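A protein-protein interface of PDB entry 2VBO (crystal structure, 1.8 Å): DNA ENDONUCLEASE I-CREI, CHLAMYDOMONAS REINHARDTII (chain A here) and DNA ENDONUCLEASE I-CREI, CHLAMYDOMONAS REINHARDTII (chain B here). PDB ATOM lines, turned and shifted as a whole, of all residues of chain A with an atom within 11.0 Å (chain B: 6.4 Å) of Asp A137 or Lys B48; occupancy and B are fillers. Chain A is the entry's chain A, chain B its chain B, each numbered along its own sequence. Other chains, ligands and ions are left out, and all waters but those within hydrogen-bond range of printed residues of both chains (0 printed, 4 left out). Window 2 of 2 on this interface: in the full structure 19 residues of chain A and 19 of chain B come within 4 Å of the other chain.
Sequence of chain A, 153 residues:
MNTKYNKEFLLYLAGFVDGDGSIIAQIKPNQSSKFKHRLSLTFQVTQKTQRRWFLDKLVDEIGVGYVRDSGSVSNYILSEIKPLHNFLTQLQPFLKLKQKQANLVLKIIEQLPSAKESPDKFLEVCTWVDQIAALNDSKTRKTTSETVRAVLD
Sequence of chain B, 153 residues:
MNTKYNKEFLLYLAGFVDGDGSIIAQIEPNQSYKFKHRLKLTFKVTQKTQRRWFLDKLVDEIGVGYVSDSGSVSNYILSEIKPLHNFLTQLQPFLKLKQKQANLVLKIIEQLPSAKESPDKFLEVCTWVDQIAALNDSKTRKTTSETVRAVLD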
ATOM      1  N   VAL A  17      15.159   6.498 -28.931  1.00  0.00           N
ATOM      2  CA  VAL A  17      14.675   7.888 -28.973  1.00  0.00           C
ATOM      3  C   VAL A  17      15.321   8.717 -27.850  1.00  0.00           C
ATOM      4  O   VAL A  17      15.767   9.875 -28.054  1.00  0.00           O
ATOM      5  CB  VAL A  17      13.158   7.895 -28.799  1.00  0.00           C
ATOM      6  CG1 VAL A  17      12.686   9.322 -28.490  1.00  0.00           C
ATOM      7  CG2 VAL A  17      12.518   7.326 -30.091  1.00  0.00           C
ATOM      8  N   ASP A  18      15.434   8.137 -26.660  1.00  0.00           N
ATOM      9  CA  ASP A  18      16.138   8.851 -25.587  1.00  0.00           C
ATOM     10  C   ASP A  18      17.560   9.144 -26.040  1.00  0.00           C
ATOM     11  O   ASP A  18      18.130  10.169 -25.652  1.00  0.00           O
ATOM     12  CB  ASP A  18      16.147   8.054 -24.279  1.00  0.00           C
ATOM     13  CG  ASP A  18      14.877   8.258 -23.451  1.00  0.00           C
ATOM     14  OD1 ASP A  18      14.116   9.241 -23.697  1.00  0.00           O
ATOM     15  OD2 ASP A  18      14.664   7.428 -22.537  1.00  0.00           O
ATOM     16  N   GLY A  19      18.098   8.298 -26.915  1.00  0.00           N
ATOM     17  CA  GLY A  19      19.448   8.523 -27.497  1.00  0.00           C
ATOM     18  C   GLY A  19      19.455   9.576 -28.613  1.00  0.00           C
ATOM     19  O   GLY A  19      19.829  10.729 -28.370  1.00  0.00           O
ATOM     20  N   ASP A  20      19.007   9.194 -29.816  1.00  0.00           N
ATOM     21  CA  ASP A  20      19.145  10.001 -31.025  1.00  0.00           C
ATOM     22  C   ASP A  20      17.838  10.702 -31.472  1.00  0.00           C
ATOM     23  O   ASP A  20      17.765  11.282 -32.568  1.00  0.00           O
ATOM     24  CB  ASP A  20      19.593   9.103 -32.195  1.00  0.00           C
ATOM     25  CG  ASP A  20      21.061   8.685 -32.126  1.00  0.00           C
ATOM     26  OD1 ASP A  20      21.889   9.385 -31.495  1.00  0.00           O
ATOM     27  OD2 ASP A  20      21.390   7.649 -32.752  1.00  0.00           O
ATOM     28  N   GLY A  21      16.779  10.584 -30.686  1.00  0.00           N
ATOM     29  CA  GLY A  21      15.505  11.180 -31.060  1.00  0.00           C
ATOM     30  C   GLY A  21      15.296  12.580 -30.474  1.00  0.00           C
ATOM     31  O   GLY A  21      16.093  13.088 -29.670  1.00  0.00           O
ATOM     32  N   SER A  22      14.193  13.203 -30.869  1.00  0.00           N
ATOM     33  CA  SER A  22      13.889  14.542 -30.415  1.00  0.00           C
ATOM     34  C   SER A  22      12.390  14.696 -30.430  1.00  0.00           C
ATOM     35  O   SER A  22      11.729  14.288 -31.392  1.00  0.00           O
ATOM     36  CB  SER A  22      14.565  15.584 -31.337  1.00  0.00           C
ATOM     37  OG  SER A  22      14.487  16.902 -30.803  1.00  0.00           O
ATOM     38  N   ILE A  23      11.842  15.278 -29.364  1.00  0.00           N
ATOM     39  CA  ILE A  23      10.391  15.559 -29.303  1.00  0.00           C
ATOM     40  C   ILE A  23      10.272  17.061 -29.201  1.00  0.00           C
ATOM     41  O   ILE A  23      10.809  17.679 -28.257  1.00  0.00           O
ATOM     42  CB  ILE A  23       9.733  14.829 -28.120  1.00  0.00           C
ATOM     43  CG1 ILE A  23       9.854  13.303 -28.336  1.00  0.00           C
ATOM     44  CG2 ILE A  23       8.262  15.300 -27.908  1.00  0.00           C
ATOM     45  CD1 ILE A  23       9.144  12.523 -27.213  1.00  0.00           C
ATOM     46  N   ILE A  24       9.667  17.648 -30.237  1.00  0.00           N
ATOM     47  CA  ILE A  24       9.873  19.073 -30.537  1.00  0.00           C
ATOM     48  C   ILE A  24       8.524  19.731 -30.582  1.00  0.00           C
ATOM     49  O   ILE A  24       7.610  19.194 -31.216  1.00  0.00           O
ATOM     50  CB  ILE A  24      10.574  19.299 -31.896  1.00  0.00           C
ATOM     51  CG1 ILE A  24      11.934  18.602 -31.904  1.00  0.00           C
ATOM     52  CG2 ILE A  24      10.766  20.823 -32.182  1.00  0.00           C
ATOM     53  CD1 ILE A  24      12.541  18.559 -33.265  1.00  0.00           C
ATOM     54  N   ALA A  25       8.382  20.880 -29.919  1.00  0.00           N
ATOM     55  CA  ALA A  25       7.175  21.668 -30.115  1.00  0.00           C
ATOM     56  C   ALA A  25       7.607  23.060 -30.543  1.00  0.00           C
ATOM     57  O   ALA A  25       8.572  23.600 -30.002  1.00  0.00           O
ATOM     58  CB  ALA A  25       6.382  21.754 -28.807  1.00  0.00           C
ATOM     59  N   GLN A  44      10.984  13.245 -33.965  1.00  0.00           N
ATOM     60  CA  GLN A  44      12.050  13.143 -34.981  1.00  0.00           C
ATOM     61  C   GLN A  44      13.088  12.120 -34.516  1.00  0.00           C
ATOM     62  O   GLN A  44      13.402  12.054 -33.332  1.00  0.00           O
ATOM     63  CB  GLN A  44      12.698  14.529 -35.198  1.00  0.00           C
ATOM     64  CG  GLN A  44      14.121  14.517 -35.774  1.00  0.00           C
ATOM     65  CD  GLN A  44      14.711  15.925 -36.010  1.00  0.00           C
ATOM     66  OE1 GLN A  44      14.175  16.734 -36.775  1.00  0.00           O
ATOM     67  NE2 GLN A  44      15.833  16.204 -35.360  1.00  0.00           N
ATOM     68  N   LEU A  97      14.353   9.767 -20.547  1.00  0.00           N
ATOM     69  CA  LEU A  97      14.920  11.122 -20.692  1.00  0.00           C
ATOM     70  C   LEU A  97      13.928  12.089 -21.331  1.00  0.00           C
ATOM     71  O   LEU A  97      13.949  13.302 -21.079  1.00  0.00           O
ATOM     72  CB  LEU A  97      16.207  11.088 -21.515  1.00  0.00           C
ATOM     73  CG  LEU A  97      17.401  10.360 -20.880  1.00  0.00           C
ATOM     74  CD1 LEU A  97      18.624  10.575 -21.768  1.00  0.00           C
ATOM     75  CD2 LEU A  97      17.681  10.924 -19.487  1.00  0.00           C
ATOM     76  N   LYS A  98      13.054  11.560 -22.174  1.00  0.00           N
ATOM     77  CA  LYS A  98      12.153  12.411 -22.966  1.00  0.00           C
ATOM     78  C   LYS A  98      10.684  12.137 -22.624  1.00  0.00           C
ATOM     79  O   LYS A  98       9.773  12.536 -23.345  1.00  0.00           O
ATOM     80  CB  LYS A  98      12.474  12.281 -24.464  1.00  0.00           C
ATOM     81  CG  LYS A  98      13.918  12.819 -24.821  1.00  0.00           C
ATOM     82  CD  LYS A  98      14.361  12.387 -26.227  1.00  0.00           C
ATOM     83  CE  LYS A  98      15.847  12.694 -26.524  1.00  0.00           C
ATOM     84  NZ  LYS A  98      15.988  14.146 -26.551  1.00  0.00           N
ATOM     85  N   GLN A 101       8.655  15.524 -22.136  1.00  0.00           N
ATOM     86  CA  GLN A 101       8.388  16.178 -23.391  1.00  0.00           C
ATOM     87  C   GLN A 101       7.243  15.417 -24.056  1.00  0.00           C
ATOM     88  O   GLN A 101       6.350  16.054 -24.581  1.00  0.00           O
ATOM     89  CB  GLN A 101       9.635  16.156 -24.297  1.00  0.00           C
ATOM     90  CG  GLN A 101      10.788  17.065 -23.844  1.00  0.00           C
ATOM     91  CD  GLN A 101      11.824  16.312 -23.003  1.00  0.00           C
ATOM     92  OE1 GLN A 101      11.454  15.554 -22.099  1.00  0.00           O
ATOM     93  NE2 GLN A 101      13.126  16.510 -23.298  1.00  0.00           N
ATOM     94  N   VAL A 129       4.540  24.788 -24.724  1.00  0.00           N
ATOM     95  CA  VAL A 129       5.597  24.651 -25.739  1.00  0.00           C
ATOM     96  C   VAL A 129       6.917  25.157 -25.133  1.00  0.00           C
ATOM     97  O   VAL A 129       7.964  24.517 -25.289  1.00  0.00           O
ATOM     98  CB  VAL A 129       5.275  25.409 -27.027  1.00  0.00           C
ATOM     99  CG1 VAL A 129       6.447  25.312 -28.005  1.00  0.00           C
ATOM    100  CG2 VAL A 129       4.005  24.873 -27.711  1.00  0.00           C
ATOM    101  N   ASP A 130       6.876  26.281 -24.415  1.00  0.00           N
ATOM    102  CA  ASP A 130       8.083  26.760 -23.722  1.00  0.00           C
ATOM    103  C   ASP A 130       8.697  25.681 -22.826  1.00  0.00           C
ATOM    104  O   ASP A 130       9.930  25.557 -22.755  1.00  0.00           O
ATOM    105  CB  ASP A 130       7.782  27.943 -22.797  1.00  0.00           C
ATOM    106  CG  ASP A 130       7.370  29.212 -23.517  1.00  0.00           C
ATOM    107  OD1 ASP A 130       7.556  29.385 -24.759  1.00  0.00           O
ATOM    108  OD2 ASP A 130       6.874  30.068 -22.740  1.00  0.00           O
ATOM    109  N   GLN A 131       7.852  24.924 -22.123  1.00  0.00           N
ATOM    110  CA  GLN A 131       8.349  23.939 -21.166  1.00  0.00           C
ATOM    111  C   GLN A 131       9.078  22.789 -21.864  1.00  0.00           C
ATOM    112  O   GLN A 131      10.071  22.274 -21.352  1.00  0.00           O
ATOM    113  CB  GLN A 131       7.206  23.406 -20.298  1.00  0.00           C
ATOM    114  CG  GLN A 131       6.775  24.434 -19.258  1.00  0.00           C
ATOM    115  CD  GLN A 131       5.410  24.159 -18.701  1.00  0.00           C
ATOM    116  OE1 GLN A 131       5.038  23.008 -18.529  1.00  0.00           O
ATOM    117  NE2 GLN A 131       4.662  25.221 -18.380  1.00  0.00           N
ATOM    118  N   ILE A 132       8.596  22.394 -23.035  1.00  0.00           N
ATOM    119  CA  ILE A 132       9.247  21.339 -23.812  1.00  0.00           C
ATOM    120  C   ILE A 132      10.634  21.820 -24.254  1.00  0.00           C
ATOM    121  O   ILE A 132      11.634  21.086 -24.131  1.00  0.00           O
ATOM    122  CB  ILE A 132       8.398  20.906 -25.023  1.00  0.00           C
ATOM    123  CG1 ILE A 132       7.104  20.190 -24.576  1.00  0.00           C
ATOM    124  CG2 ILE A 132       9.234  19.996 -25.962  1.00  0.00           C
ATOM    125  CD1 ILE A 132       6.081  20.017 -25.736  1.00  0.00           C
ATOM    126  N   ALA A 133      10.707  23.059 -24.742  1.00  0.00           N
ATOM    127  CA  ALA A 133      11.983  23.624 -25.197  1.00  0.00           C
ATOM    128  C   ALA A 133      12.961  23.672 -24.038  1.00  0.00           C
ATOM    129  O   ALA A 133      14.142  23.349 -24.220  1.00  0.00           O
ATOM    130  CB  ALA A 133      11.766  25.059 -25.808  1.00  0.00           C
ATOM    131  N   ALA A 134      12.485  24.043 -22.846  1.00  0.00           N
ATOM    132  CA  ALA A 134      13.345  24.025 -21.643  1.00  0.00           C
ATOM    133  C   ALA A 134      13.892  22.646 -21.331  1.00  0.00           C
ATOM    134  O   ALA A 134      15.057  22.508 -20.973  1.00  0.00           O
ATOM    135  CB  ALA A 134      12.615  24.562 -20.422  1.00  0.00           C
ATOM    136  N   LEU A 135      13.038  21.629 -21.393  1.00  0.00           N
ATOM    137  CA  LEU A 135      13.505  20.245 -21.165  1.00  0.00           C
ATOM    138  C   LEU A 135      14.532  19.774 -22.196  1.00  0.00           C
ATOM    139  O   LEU A 135      15.470  19.046 -21.871  1.00  0.00           O
ATOM    140  CB  LEU A 135      12.303  19.306 -21.141  1.00  0.00           C
ATOM    141  CG  LEU A 135      11.379  19.554 -19.932  1.00  0.00           C
ATOM    142  CD1 LEU A 135       9.998  18.946 -20.207  1.00  0.00           C
ATOM    143  CD2 LEU A 135      12.046  18.865 -18.712  1.00  0.00           C
ATOM    144  N   ASN A 136      14.345  20.194 -23.438  1.00  0.00           N
ATOM    145  CA  ASN A 136      15.274  19.863 -24.536  1.00  0.00           C
ATOM    146  C   ASN A 136      16.599  20.621 -24.351  1.00  0.00           C
ATOM    147  O   ASN A 136      16.687  21.483 -23.459  1.00  0.00           O
ATOM    148  CB  ASN A 136      14.618  20.237 -25.867  1.00  0.00           C
ATOM    149  CG  ASN A 136      13.532  19.257 -26.286  1.00  0.00           C
ATOM    150  OD1 ASN A 136      13.368  18.188 -25.673  1.00  0.00           O
ATOM    151  ND2 ASN A 136      12.767  19.621 -27.320  1.00  0.00           N
ATOM    152  N   ASP A 137      17.612  20.333 -25.177  1.00  0.00           N
ATOM    153  CA  ASP A 137      18.847  21.126 -25.200  1.00  0.00           C
ATOM    154  C   ASP A 137      18.646  22.246 -26.221  1.00  0.00           C
ATOM    155  O   ASP A 137      19.245  22.224 -27.302  1.00  0.00           O
ATOM    156  CB  ASP A 137      20.059  20.249 -25.556  1.00  0.00           C
ATOM    157  CG  ASP A 137      20.333  19.166 -24.487  1.00  0.00           C
ATOM    158  OD1 ASP A 137      20.084  19.415 -23.271  1.00  0.00           O
ATOM    159  OD2 ASP A 137      20.806  18.060 -24.854  1.00  0.00           O
ATOM    160  N   SER A 138      17.752  23.182 -25.910  1.00  0.00           N
ATOM    161  CA  SER A 138      17.380  24.244 -26.854  1.00  0.00           C
ATOM    162  C   SER A 138      18.508  25.246 -27.030  1.00  0.00           C
ATOM    163  O   SER A 138      19.055  25.709 -26.020  1.00  0.00           O
ATOM    164  CB  SER A 138      16.144  25.004 -26.347  1.00  0.00           C
ATOM    165  OG  SER A 138      15.714  25.924 -27.336  1.00  0.00           O
ATOM    166  N   LYS A 139      18.807  25.634 -28.278  1.00  0.00           N
ATOM    167  CA  LYS A 139      19.950  26.507 -28.540  1.00  0.00           C
ATOM    168  C   LYS A 139      19.743  27.522 -29.676  1.00  0.00           C
ATOM    169  O   LYS A 139      20.543  28.458 -29.829  1.00  0.00           O
ATOM    170  CB  LYS A 139      21.182  25.671 -28.881  1.00  0.00           C
ATOM    171  CG  LYS A 139      21.754  24.815 -27.724  1.00  0.00           C
ATOM    172  CD  LYS A 139      23.051  24.102 -28.155  1.00  0.00           C
ATOM    173  CE  LYS A 139      22.766  22.917 -29.071  1.00  0.00           C
ATOM    174  NZ  LYS A 139      22.020  21.814 -28.368  1.00  0.00           N
ATOM    175  N   THR A 140      18.727  27.301 -30.509  1.00  0.00           N
ATOM    176  CA  THR A 140      18.451  28.204 -31.648  1.00  0.00           C
ATOM    177  C   THR A 140      17.012  28.711 -31.726  1.00  0.00           C
ATOM    178  O   THR A 140      16.538  29.096 -32.813  1.00  0.00           O
ATOM    179  CB  THR A 140      18.833  27.613 -33.020  1.00  0.00           C
ATOM    180  OG1 THR A 140      18.077  26.426 -33.304  1.00  0.00           O
ATOM    181  CG2 THR A 140      20.337  27.297 -33.098  1.00  0.00           C
ATOM    182  N   ARG A 141      16.331  28.726 -30.584  1.00  0.00           N
ATOM    183  CA  ARG A 141      14.888  28.992 -30.519  1.00  0.00           C
ATOM    184  C   ARG A 141      14.670  30.489 -30.647  1.00  0.00           C
ATOM    185  O   ARG A 141      15.431  31.276 -30.054  1.00  0.00           O
ATOM    186  CB  ARG A 141      14.340  28.527 -29.158  1.00  0.00           C
ATOM    187  CG  ARG A 141      12.812  28.578 -29.041  1.00  0.00           C
ATOM    188  CD  ARG A 141      12.321  27.707 -27.885  1.00  0.00           C
ATOM    189  NE  ARG A 141      10.863  27.668 -27.862  1.00  0.00           N
ATOM    190  CZ  ARG A 141      10.108  28.223 -26.915  1.00  0.00           C
ATOM    191  NH1 ARG A 141      10.653  28.861 -25.863  1.00  0.00           N
ATOM    192  NH2 ARG A 141       8.792  28.137 -27.027  1.00  0.00           N
ATOM    193  N   THR B  46      27.980   8.020 -23.799  1.00  0.00           N
ATOM    194  CA  THR B  46      28.281   9.458 -23.588  1.00  0.00           C
ATOM    195  C   THR B  46      26.987  10.216 -23.341  1.00  0.00           C
ATOM    196  O   THR B  46      25.964   9.863 -23.930  1.00  0.00           O
ATOM    197  CB  THR B  46      28.954  10.072 -24.850  1.00  0.00           C
ATOM    198  OG1 THR B  46      30.078   9.266 -25.235  1.00  0.00           O
ATOM    199  CG2 THR B  46      29.417  11.529 -24.587  1.00  0.00           C
ATOM    200  N   GLN B  47      27.030  11.255 -22.502  1.00  0.00           N
ATOM    201  CA  GLN B  47      25.866  12.127 -22.265  1.00  0.00           C
ATOM    202  C   GLN B  47      26.334  13.459 -21.688  1.00  0.00           C
ATOM    203  O   GLN B  47      27.251  13.498 -20.881  1.00  0.00           O
ATOM    204  CB  GLN B  47      24.847  11.489 -21.289  1.00  0.00           C
ATOM    205  CG  GLN B  47      23.401  12.021 -21.400  1.00  0.00           C
ATOM    206  CD  GLN B  47      22.655  11.627 -22.707  1.00  0.00           C
ATOM    207  OE1 GLN B  47      21.564  12.146 -22.976  1.00  0.00           O
ATOM    208  NE2 GLN B  47      23.229  10.705 -23.501  1.00  0.00           N
ATOM    209  N   LYS B  48      25.700  14.540 -22.128  1.00  0.00           N
ATOM    210  CA  LYS B  48      25.896  15.853 -21.535  1.00  0.00           C
ATOM    211  C   LYS B  48      25.865  15.726 -20.019  1.00  0.00           C
ATOM    212  O   LYS B  48      25.026  14.994 -19.462  1.00  0.00           O
ATOM    213  CB  LYS B  48      24.768  16.779 -22.029  1.00  0.00           C
ATOM    214  CG  LYS B  48      24.960  18.253 -21.781  1.00  0.00           C
ATOM    215  CD  LYS B  48      23.881  19.031 -22.565  1.00  0.00           C
ATOM    216  CE  LYS B  48      23.659  20.428 -21.982  1.00  0.00           C
ATOM    217  NZ  LYS B  48      22.610  21.174 -22.760  1.00  0.00           N
ATOM    218  N   THR B  49      26.795  16.410 -19.353  1.00  0.00           N
ATOM    219  CA  THR B  49      27.014  16.236 -17.911  1.00  0.00           C
ATOM    220  C   THR B  49      25.781  16.612 -17.078  1.00  0.00           C
ATOM    221  O   THR B  49      25.551  16.053 -15.983  1.00  0.00           O
ATOM    222  CB  THR B  49      28.291  17.003 -17.492  1.00  0.00           C
ATOM    223  OG1 THR B  49      29.410  16.425 -18.174  1.00  0.00           O
ATOM    224  CG2 THR B  49      28.555  16.937 -15.974  1.00  0.00           C
ATOM    225  N   GLN B  50      24.963  17.527 -17.605  1.00  0.00           N
ATOM    226  CA  GLN B  50      23.652  17.828 -17.018  1.00  0.00           C
ATOM    227  C   GLN B  50      22.867  16.548 -16.724  1.00  0.00           C
ATOM    228  O   GLN B  50      22.113  16.460 -15.738  1.00  0.00           O
ATOM    229  CB  GLN B  50      22.901  18.720 -18.010  1.00  0.00           C
ATOM    230  CG  GLN B  50      21.456  18.966 -17.756  1.00  0.00           C
ATOM    231  CD  GLN B  50      20.888  19.981 -18.757  1.00  0.00           C
ATOM    232  OE1 GLN B  50      21.503  21.018 -19.040  1.00  0.00           O
ATOM    233  NE2 GLN B  50      19.719  19.686 -19.290  1.00  0.00           N
ATOM    234  N   ARG B  51      23.039  15.553 -17.588  1.00  0.00           N
ATOM    235  CA  ARG B  51      22.335  14.274 -17.436  1.00  0.00           C
ATOM    236  C   ARG B  51      23.237  13.151 -16.938  1.00  0.00           C
ATOM    237  O   ARG B  51      22.931  11.965 -17.108  1.00  0.00           O
ATOM    238  CB  ARG B  51      21.725  13.864 -18.769  1.00  0.00           C
ATOM    239  CG  ARG B  51      20.470  14.701 -19.116  1.00  0.00           C
ATOM    240  CD  ARG B  51      19.814  14.231 -20.442  1.00  0.00           C
ATOM    241  NE  ARG B  51      20.640  14.528 -21.629  1.00  0.00           N
ATOM    242  CZ  ARG B  51      20.709  15.716 -22.233  1.00  0.00           C
ATOM    243  NH1 ARG B  51      20.018  16.762 -21.767  1.00  0.00           N
ATOM    244  NH2 ARG B  51      21.468  15.847 -23.321  1.00  0.00           N
ATOM    245  N   ARG B  52      24.339  13.503 -16.292  1.00  0.00           N
ATOM    246  CA  ARG B  52      25.198  12.467 -15.729  1.00  0.00           C
ATOM    247  C   ARG B  52      24.411  11.525 -14.810  1.00  0.00           C
ATOM    248  O   ARG B  52      24.744  10.355 -14.693  1.00  0.00           O
ATOM    249  CB  ARG B  52      26.332  13.174 -14.990  1.00  0.00           C
ATOM    250  CG  ARG B  52      27.301  12.290 -14.359  1.00  0.00           C
ATOM    251  CD  ARG B  52      27.790  12.940 -13.086  1.00  0.00           C
ATOM    252  NE  ARG B  52      28.408  11.800 -12.448  1.00  0.00           N
ATOM    253  CZ  ARG B  52      29.696  11.704 -12.183  1.00  0.00           C
ATOM    254  NH1 ARG B  52      30.501  12.741 -12.391  1.00  0.00           N
ATOM    255  NH2 ARG B  52      30.136  10.588 -11.639  1.00  0.00           N
ATOM    256  N   TRP B  53      23.355  12.025 -14.171  1.00  0.00           N
ATOM    257  CA  TRP B  53      22.558  11.205 -13.261  1.00  0.00           C
ATOM    258  C   TRP B  53      22.124   9.915 -13.943  1.00  0.00           C
ATOM    259  O   TRP B  53      22.037   8.869 -13.309  1.00  0.00           O
ATOM    260  CB  TRP B  53      21.333  11.964 -12.719  1.00  0.00           C
ATOM    261  CG  TRP B  53      20.309  12.337 -13.748  1.00  0.00           C
ATOM    262  CD1 TRP B  53      20.241  13.511 -14.451  1.00  0.00           C
ATOM    263  CD2 TRP B  53      19.231  11.525 -14.209  1.00  0.00           C
ATOM    264  NE1 TRP B  53      19.161  13.486 -15.311  1.00  0.00           N
ATOM    265  CE2 TRP B  53      18.513  12.287 -15.162  1.00  0.00           C
ATOM    266  CE3 TRP B  53      18.754  10.247 -13.862  1.00  0.00           C
ATOM    267  CZ2 TRP B  53      17.391  11.789 -15.821  1.00  0.00           C
ATOM    268  CZ3 TRP B  53      17.630   9.767 -14.498  1.00  0.00           C
ATOM    269  CH2 TRP B  53      16.961  10.528 -15.476  1.00  0.00           C
ATOM    270  N   LEU B  55      23.768   8.274 -16.308  1.00  0.00           N
ATOM    271  CA  LEU B  55      24.957   7.446 -16.315  1.00  0.00           C
ATOM    272  C   LEU B  55      25.264   6.823 -14.934  1.00  0.00           C
ATOM    273  O   LEU B  55      25.601   5.625 -14.828  1.00  0.00           O
ATOM    274  CB  LEU B  55      26.152   8.278 -16.829  1.00  0.00           C
ATOM    275  CG  LEU B  55      25.958   8.921 -18.218  1.00  0.00           C
ATOM    276  CD1 LEU B  55      27.196   9.691 -18.645  1.00  0.00           C
ATOM    277  CD2 LEU B  55      25.610   7.849 -19.291  1.00  0.00           C
ATOM    278  N   SER B  72      32.139  19.184 -20.258  1.00  0.00           N
ATOM    279  CA  SER B  72      30.856  19.402 -20.933  1.00  0.00           C
ATOM    280  C   SER B  72      30.007  18.117 -21.030  1.00  0.00           C
ATOM    281  O   SER B  72      28.762  18.155 -21.005  1.00  0.00           O
ATOM    282  CB  SER B  72      31.140  20.014 -22.320  1.00  0.00           C
ATOM    283  OG  SER B  72      30.036  19.921 -23.211  1.00  0.00           O
ATOM    284  N   VAL B  73      30.690  16.984 -21.177  1.00  0.00           N
ATOM    285  CA  VAL B  73      30.040  15.684 -21.250  1.00  0.00           C
ATOM    286  C   VAL B  73      30.712  14.709 -20.300  1.00  0.00           C
ATOM    287  O   VAL B  73      31.877  14.892 -19.887  1.00  0.00           O
ATOM    288  CB  VAL B  73      29.971  15.073 -22.689  1.00  0.00           C
ATOM    289  CG1 VAL B  73      29.289  16.035 -23.672  1.00  0.00           C
ATOM    290  CG2 VAL B  73      31.345  14.629 -23.191  1.00  0.00           C
ATOM    291  N   SER B  74      29.960  13.665 -19.981  1.00  0.00           N
ATOM    292  CA  SER B  74      30.402  12.585 -19.111  1.00  0.00           C
ATOM    293  C   SER B  74      30.241  11.274 -19.894  1.00  0.00           C
ATOM    294  O   SER B  74      29.506  11.208 -20.878  1.00  0.00           O
ATOM    295  CB  SER B  74      29.517  12.554 -17.861  1.00  0.00           C
ATOM    296  OG  SER B  74      29.628  13.774 -17.109  1.00  0.00           O
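Of the printed residues of chain B, Leu A97 touches Gln B47 and Trp B53. Asp A130 touches none of the printed residues of chain B. Printed residues of chain B within 4 Å of Asp A137: Lys B48 (3.1 Å) and Arg B51 (2.8 Å). Of the printed residues of chain A, Gln B47 touches Leu A97 (3.5 Å). Of chain A, only Asp A137 (3.1 Å) comes within 4 Å of Lys B48. No residue of chain A comes within 4 Å of Thr B49. Arg B51 touches just one residue of chain A: Asp A137 (2.8 Å). Of the printed residues of chain A, Trp B53 touches Leu A97 (3.8 Å). No residue of chain A comes within 4 Å of Val B73. No residue of chain A comes within 4 Å of Ser B74. The nearest printed residue of chain B that does not touch Asp A137 is Gln B50 (4.01 Å).
Of the 26 printed residues of chain A, 2 touch a printed residue of chain B. Printed residues of chain A that touch a printed residue of chain B: Leu A97 and Asp A137.
OE1 of Gln B47 touches CD1 of Leu A97, at 3.5 Å. CD2 of Leu A97 touches CZ2 of Trp B53, at 3.8 Å.
NH2 of Arg B51 lies within salt-bridge range of OD2 of Asp A137 (2.8 Å). OD1 of Asp A137 lies within salt-bridge range of NZ of Lys B48 (3.1 Å).
The guanidinium group (NE) of Arg B51 sits at hydrogen-bond distance from the side-chain amide oxygen (OE1) of Gln B47 (2.9 Å). The backbone carbonyl oxygen (O) of Gln B47 lies within hydrogen-bond range of the backbone NH (N) of Ser B74, at 2.9 Å. O of Asp A137 lies within hydrogen-bond range of NZ of Lys A139, at 3.0 Å. OD2 of Asp A18 sits at hydrogen-bond distance from N of Leu A97, at 3.1 Å.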
